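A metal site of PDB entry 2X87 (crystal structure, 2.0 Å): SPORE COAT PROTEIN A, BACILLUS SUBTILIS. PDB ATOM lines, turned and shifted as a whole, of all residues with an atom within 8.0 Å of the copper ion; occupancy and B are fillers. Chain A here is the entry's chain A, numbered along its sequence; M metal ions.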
ATOM      1  N   PRO A 226      -2.212  13.138  29.121  1.00  0.00           N
ATOM      2  CA  PRO A 226      -2.711  11.861  28.583  1.00  0.00           C
ATOM      3  C   PRO A 226      -3.555  11.994  27.305  1.00  0.00           C
ATOM      4  O   PRO A 226      -3.900  10.990  26.686  1.00  0.00           O
ATOM      5  CB  PRO A 226      -3.560  11.295  29.726  1.00  0.00           C
ATOM      6  CG  PRO A 226      -3.990  12.494  30.506  1.00  0.00           C
ATOM      7  CD  PRO A 226      -2.942  13.551  30.338  1.00  0.00           C
ATOM      8  N   LEU A 374      -5.020  -3.884  27.392  1.00  0.00           N
ATOM      9  CA  LEU A 374      -4.714  -2.456  27.384  1.00  0.00           C
ATOM     10  C   LEU A 374      -4.858  -1.985  28.815  1.00  0.00           C
ATOM     11  O   LEU A 374      -5.961  -1.947  29.358  1.00  0.00           O
ATOM     12  CB  LEU A 374      -5.660  -1.707  26.432  1.00  0.00           C
ATOM     13  CG  LEU A 374      -5.790  -2.270  25.009  1.00  0.00           C
ATOM     14  CD1 LEU A 374      -6.679  -1.398  24.113  1.00  0.00           C
ATOM     15  CD2 LEU A 374      -4.432  -2.508  24.350  1.00  0.00           C
ATOM     16  N   ALA A 375      -3.743  -1.634  29.442  1.00  0.00           N
ATOM     17  CA  ALA A 375      -3.735  -1.309  30.854  1.00  0.00           C
ATOM     18  C   ALA A 375      -2.789  -0.167  31.168  1.00  0.00           C
ATOM     19  O   ALA A 375      -2.723   0.824  30.434  1.00  0.00           O
ATOM     20  CB  ALA A 375      -3.385  -2.558  31.685  1.00  0.00           C
ATOM     21  N   LEU A 386       0.295   4.616  30.457  1.00  0.00           N
ATOM     22  CA  LEU A 386      -0.523   3.655  29.709  1.00  0.00           C
ATOM     23  C   LEU A 386       0.369   2.555  29.141  1.00  0.00           C
ATOM     24  O   LEU A 386       1.392   2.833  28.531  1.00  0.00           O
ATOM     25  CB  LEU A 386      -1.338   4.365  28.620  1.00  0.00           C
ATOM     26  CG  LEU A 386      -2.390   5.354  29.151  1.00  0.00           C
ATOM     27  CD1 LEU A 386      -1.803   6.754  29.387  1.00  0.00           C
ATOM     28  CD2 LEU A 386      -3.557   5.452  28.199  1.00  0.00           C
ATOM     29  N   LEU A 387      -0.027   1.307  29.377  1.00  0.00           N
ATOM     30  CA  LEU A 387       0.812   0.151  29.036  1.00  0.00           C
ATOM     31  C   LEU A 387       0.084  -0.929  28.245  1.00  0.00           C
ATOM     32  O   LEU A 387      -1.092  -1.199  28.460  1.00  0.00           O
ATOM     33  CB  LEU A 387       1.425  -0.460  30.309  1.00  0.00           C
ATOM     34  CG  LEU A 387       2.353   0.408  31.167  1.00  0.00           C
ATOM     35  CD1 LEU A 387       2.856  -0.381  32.387  1.00  0.00           C
ATOM     36  CD2 LEU A 387       3.517   0.962  30.361  1.00  0.00           C
ATOM     37  N   LEU A 388       0.802  -1.545  27.318  1.00  0.00           N
ATOM     38  CA  LEU A 388       0.328  -2.721  26.609  1.00  0.00           C
ATOM     39  C   LEU A 388       0.826  -3.947  27.393  1.00  0.00           C
ATOM     40  O   LEU A 388       2.033  -4.108  27.583  1.00  0.00           O
ATOM     41  CB  LEU A 388       0.868  -2.747  25.177  1.00  0.00           C
ATOM     42  CG  LEU A 388       0.534  -1.552  24.263  1.00  0.00           C
ATOM     43  CD1 LEU A 388       1.365  -1.597  22.978  1.00  0.00           C
ATOM     44  CD2 LEU A 388      -0.943  -1.503  23.949  1.00  0.00           C
ATOM     45  N   ASN A 413      -9.769  -4.504  26.162  1.00  0.00           N
ATOM     46  CA  ASN A 413      -9.772  -3.117  26.610  1.00  0.00           C
ATOM     47  C   ASN A 413     -10.691  -2.908  27.803  1.00  0.00           C
ATOM     48  O   ASN A 413     -11.885  -2.684  27.624  1.00  0.00           O
ATOM     49  CB  ASN A 413     -10.152  -2.160  25.463  1.00  0.00           C
ATOM     50  CG  ASN A 413     -10.052  -0.693  25.870  1.00  0.00           C
ATOM     51  OD1 ASN A 413      -9.665  -0.368  26.985  1.00  0.00           O
ATOM     52  ND2 ASN A 413     -10.405   0.198  24.951  1.00  0.00           N
ATOM     53  N   THR A 415     -10.271  -0.341  29.819  1.00  0.00           N
ATOM     54  CA  THR A 415     -10.168   1.081  30.168  1.00  0.00           C
ATOM     55  C   THR A 415     -11.448   1.803  29.791  1.00  0.00           C
ATOM     56  O   THR A 415     -12.347   1.213  29.175  1.00  0.00           O
ATOM     57  CB  THR A 415      -8.957   1.773  29.486  1.00  0.00           C
ATOM     58  OG1 THR A 415      -9.218   1.932  28.084  1.00  0.00           O
ATOM     59  CG2 THR A 415      -7.666   0.982  29.697  1.00  0.00           C
ATOM     60  N   GLY A 417     -11.785   4.355  27.692  1.00  0.00           N
ATOM     61  CA  GLY A 417     -11.813   4.903  26.327  1.00  0.00           C
ATOM     62  C   GLY A 417     -11.354   3.977  25.211  1.00  0.00           C
ATOM     63  O   GLY A 417     -10.843   2.880  25.465  1.00  0.00           O
ATOM     64  N   THR A 418     -11.569   4.427  23.974  1.00  0.00           N
ATOM     65  CA  THR A 418     -11.114   3.716  22.793  1.00  0.00           C
ATOM     66  C   THR A 418      -9.624   3.952  22.551  1.00  0.00           C
ATOM     67  O   THR A 418      -9.107   5.041  22.805  1.00  0.00           O
ATOM     68  CB  THR A 418     -11.902   4.163  21.536  1.00  0.00           C
ATOM     69  OG1 THR A 418     -13.282   3.838  21.719  1.00  0.00           O
ATOM     70  CG2 THR A 418     -11.403   3.444  20.294  1.00  0.00           C
ATOM     71  N   HIS A 419      -8.933   2.913  22.077  1.00  0.00           N
ATOM     72  CA  HIS A 419      -7.551   3.032  21.653  1.00  0.00           C
ATOM     73  C   HIS A 419      -7.408   2.544  20.217  1.00  0.00           C
ATOM     74  O   HIS A 419      -7.780   1.406  19.924  1.00  0.00           O
ATOM     75  CB  HIS A 419      -6.620   2.239  22.578  1.00  0.00           C
ATOM     76  CG  HIS A 419      -6.677   2.676  24.002  1.00  0.00           C
ATOM     77  ND1 HIS A 419      -5.884   3.679  24.505  1.00  0.00           N
ATOM     78  CD2 HIS A 419      -7.447   2.247  25.032  1.00  0.00           C
ATOM     79  CE1 HIS A 419      -6.154   3.852  25.784  1.00  0.00           C
ATOM     80  NE2 HIS A 419      -7.096   2.993  26.136  1.00  0.00           N
ATOM     81  N   PRO A 420      -6.893   3.418  19.319  1.00  0.00           N
ATOM     82  CA  PRO A 420      -6.609   2.987  17.964  1.00  0.00           C
ATOM     83  C   PRO A 420      -5.293   2.216  17.947  1.00  0.00           C
ATOM     84  O   PRO A 420      -4.216   2.810  18.050  1.00  0.00           O
ATOM     85  CB  PRO A 420      -6.523   4.318  17.182  1.00  0.00           C
ATOM     86  CG  PRO A 420      -6.028   5.308  18.208  1.00  0.00           C
ATOM     87  CD  PRO A 420      -6.543   4.828  19.554  1.00  0.00           C
ATOM     88  N   ILE A 421      -5.392   0.897  17.872  1.00  0.00           N
ATOM     89  CA  ILE A 421      -4.210   0.056  17.953  1.00  0.00           C
ATOM     90  C   ILE A 421      -3.620  -0.120  16.569  1.00  0.00           C
ATOM     91  O   ILE A 421      -4.329  -0.462  15.620  1.00  0.00           O
ATOM     92  CB  ILE A 421      -4.496  -1.318  18.630  1.00  0.00           C
ATOM     93  CG1 ILE A 421      -5.033  -1.118  20.051  1.00  0.00           C
ATOM     94  CG2 ILE A 421      -3.231  -2.219  18.601  1.00  0.00           C
ATOM     95  CD1 ILE A 421      -4.154  -0.254  20.988  1.00  0.00           C
ATOM     96  N   ALA A 469     -10.116  -0.159  19.253  1.00  0.00           N
ATOM     97  CA  ALA A 469     -10.436  -1.097  20.317  1.00  0.00           C
ATOM     98  C   ALA A 469     -11.250  -0.342  21.362  1.00  0.00           C
ATOM     99  O   ALA A 469     -10.681   0.389  22.185  1.00  0.00           O
ATOM    100  CB  ALA A 469      -9.162  -1.667  20.927  1.00  0.00           C
ATOM    101  N   HIS A 491       1.500  -0.419  18.785  1.00  0.00           N
ATOM    102  CA  HIS A 491       1.227   0.649  19.731  1.00  0.00           C
ATOM    103  C   HIS A 491      -0.155   1.260  19.559  1.00  0.00           C
ATOM    104  O   HIS A 491      -0.820   1.062  18.543  1.00  0.00           O
ATOM    105  CB  HIS A 491       2.289   1.765  19.643  1.00  0.00           C
ATOM    106  CG  HIS A 491       2.413   2.421  18.298  1.00  0.00           C
ATOM    107  ND1 HIS A 491       1.786   3.601  17.984  1.00  0.00           N
ATOM    108  CD2 HIS A 491       3.119   2.074  17.199  1.00  0.00           C
ATOM    109  CE1 HIS A 491       2.087   3.953  16.750  1.00  0.00           C
ATOM    110  NE2 HIS A 491       2.910   3.040  16.255  1.00  0.00           N
ATOM    111  N   CYS A 492      -0.572   2.004  20.580  1.00  0.00           N
ATOM    112  CA  CYS A 492      -1.725   2.866  20.449  1.00  0.00           C
ATOM    113  C   CYS A 492      -1.302   4.113  19.677  1.00  0.00           C
ATOM    114  O   CYS A 492      -0.220   4.657  19.913  1.00  0.00           O
ATOM    115  CB  CYS A 492      -2.246   3.266  21.824  1.00  0.00           C
ATOM    116  SG  CYS A 492      -3.565   4.445  21.696  1.00  0.00           S
ATOM    117  N   HIS A 493      -2.149   4.550  18.748  1.00  0.00           N
ATOM    118  CA  HIS A 493      -1.798   5.693  17.911  1.00  0.00           C
ATOM    119  C   HIS A 493      -2.352   7.024  18.443  1.00  0.00           C
ATOM    120  O   HIS A 493      -2.307   8.041  17.757  1.00  0.00           O
ATOM    121  CB  HIS A 493      -2.143   5.455  16.421  1.00  0.00           C
ATOM    122  CG  HIS A 493      -1.119   6.022  15.470  1.00  0.00           C
ATOM    123  ND1 HIS A 493      -0.946   7.380  15.291  1.00  0.00           N
ATOM    124  CD2 HIS A 493      -0.225   5.416  14.655  1.00  0.00           C
ATOM    125  CE1 HIS A 493       0.018   7.581  14.413  1.00  0.00           C
ATOM    126  NE2 HIS A 493       0.476   6.404  14.007  1.00  0.00           N
ATOM    127  N   ILE A 494      -2.854   7.012  19.678  1.00  0.00           N
ATOM    128  CA  ILE A 494      -3.005   8.274  20.400  1.00  0.00           C
ATOM    129  C   ILE A 494      -1.604   8.607  20.876  1.00  0.00           C
ATOM    130  O   ILE A 494      -1.014   7.888  21.694  1.00  0.00           O
ATOM    131  CB  ILE A 494      -4.010   8.193  21.579  1.00  0.00           C
ATOM    132  CG1 ILE A 494      -5.425   7.993  21.043  1.00  0.00           C
ATOM    133  CG2 ILE A 494      -3.920   9.486  22.458  1.00  0.00           C
ATOM    134  CD1 ILE A 494      -6.451   7.583  22.067  1.00  0.00           C
ATOM    135  N   LEU A 495      -1.048   9.677  20.325  1.00  0.00           N
ATOM    136  CA  LEU A 495       0.363   9.989  20.477  1.00  0.00           C
ATOM    137  C   LEU A 495       0.767  10.268  21.920  1.00  0.00           C
ATOM    138  O   LEU A 495       1.861   9.889  22.348  1.00  0.00           O
ATOM    139  CB  LEU A 495       0.772  11.125  19.527  1.00  0.00           C
ATOM    140  CG  LEU A 495       0.542  10.837  18.033  1.00  0.00           C
ATOM    141  CD1 LEU A 495       1.171  11.936  17.209  1.00  0.00           C
ATOM    142  CD2 LEU A 495       1.070   9.458  17.602  1.00  0.00           C
ATOM    143  N   GLU A 496      -0.138  10.898  22.667  1.00  0.00           N
ATOM    144  CA  GLU A 496       0.042  11.143  24.092  1.00  0.00           C
ATOM    145  C   GLU A 496       0.128   9.813  24.889  1.00  0.00           C
ATOM    146  O   GLU A 496       0.802   9.752  25.921  1.00  0.00           O
ATOM    147  CB  GLU A 496      -1.109  12.022  24.614  1.00  0.00           C
ATOM    148  CG  GLU A 496      -0.989  13.516  24.257  1.00  0.00           C
ATOM    149  CD  GLU A 496      -1.137  13.836  22.755  1.00  0.00           C
ATOM    150  OE1 GLU A 496      -1.837  13.082  22.049  1.00  0.00           O
ATOM    151  OE2 GLU A 496      -0.554  14.845  22.297  1.00  0.00           O
ATOM    152  N   HIS A 497      -0.538   8.772  24.396  1.00  0.00           N
ATOM    153  CA  HIS A 497      -0.460   7.424  25.000  1.00  0.00           C
ATOM    154  C   HIS A 497       0.807   6.700  24.568  1.00  0.00           C
ATOM    155  O   HIS A 497       1.519   6.117  25.401  1.00  0.00           O
ATOM    156  CB  HIS A 497      -1.667   6.571  24.593  1.00  0.00           C
ATOM    157  CG  HIS A 497      -2.973   7.088  25.105  1.00  0.00           C
ATOM    158  ND1 HIS A 497      -4.163   6.411  24.903  1.00  0.00           N
ATOM    159  CD2 HIS A 497      -3.279   8.206  25.807  1.00  0.00           C
ATOM    160  CE1 HIS A 497      -5.148   7.096  25.458  1.00  0.00           C
ATOM    161  NE2 HIS A 497      -4.649   8.186  26.011  1.00  0.00           N
ATOM    162  N   GLU A 498       1.059   6.730  23.257  1.00  0.00           N
ATOM    163  CA  GLU A 498       2.238   6.112  22.647  1.00  0.00           C
ATOM    164  C   GLU A 498       3.544   6.521  23.346  1.00  0.00           C
ATOM    165  O   GLU A 498       4.410   5.675  23.574  1.00  0.00           O
ATOM    166  CB  GLU A 498       2.295   6.491  21.165  1.00  0.00           C
ATOM    167  CG  GLU A 498       3.502   5.972  20.407  1.00  0.00           C
ATOM    168  CD  GLU A 498       3.475   6.337  18.942  1.00  0.00           C
ATOM    169  OE1 GLU A 498       2.370   6.515  18.368  1.00  0.00           O
ATOM    170  OE2 GLU A 498       4.563   6.427  18.351  1.00  0.00           O
ATOM    171  N   MET A 502       2.601   3.472  25.796  1.00  0.00           N
ATOM    172  CA  MET A 502       1.722   2.467  25.208  1.00  0.00           C
ATOM    173  C   MET A 502       2.219   1.983  23.841  1.00  0.00           C
ATOM    174  O   MET A 502       1.542   2.103  22.818  1.00  0.00           O
ATOM    175  CB  MET A 502       0.295   3.005  25.140  1.00  0.00           C
ATOM    176  CG  MET A 502      -0.788   1.951  25.099  1.00  0.00           C
ATOM    177  SD  MET A 502      -2.406   2.706  25.305  1.00  0.00           S
ATOM    178  CE  MET A 502      -3.479   1.273  25.298  1.00  0.00           C
HETATM  179 CU    CU M   1      -4.343   4.756  23.796  1.00  0.00          CU
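The copper ion is bound by ND1 of His 497 (2.0 Å), ND1 of His 419 (2.0 Å) and SG of Cys 492 (2.3 Å).
The backbone carbonyl oxygen of His 419 is in hydrogen-bond range of the backbone NH of Ala 469.
The backbone carbonyl oxygen (O) of Leu 386 sits at hydrogen-bond distance from the backbone NH (N) of Met 502, 3.1 Å away.
The side-chain sulfur (SG) of Cys 492 lies close to the backbone NH (N) of Ile 494, at 3.3 Å.
A ring nitrogen (ND1) of His 419 lies close to the side-chain sulfur of Met 502 (3.7 Å).
The backbone NH (N) of Cys 492 is in hydrogen-bond range of the backbone carbonyl oxygen (O) of Met 502 (3.1 Å).
The side-chain hydroxyl of Thr 415 is in hydrogen-bond range of a ring nitrogen (NE2) of His 419, 3.1 Å away.
The backbone carbonyl oxygen (O) of Pro 226 sits at hydrogen-bond distance from a ring nitrogen (NE2) of His 497, at 3.0 Å.
The backbone carbonyl oxygen (O) of His 497 is in hydrogen-bond range of the backbone NH (N) of Met 502 (2.9 Å).
CD1 of Ile 494 touches the copper ion, 3.9 Å away.
Met 502 touches the copper ion.
The nearest printed residue that does not touch the copper ion is Leu 386 (4.5 Å).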
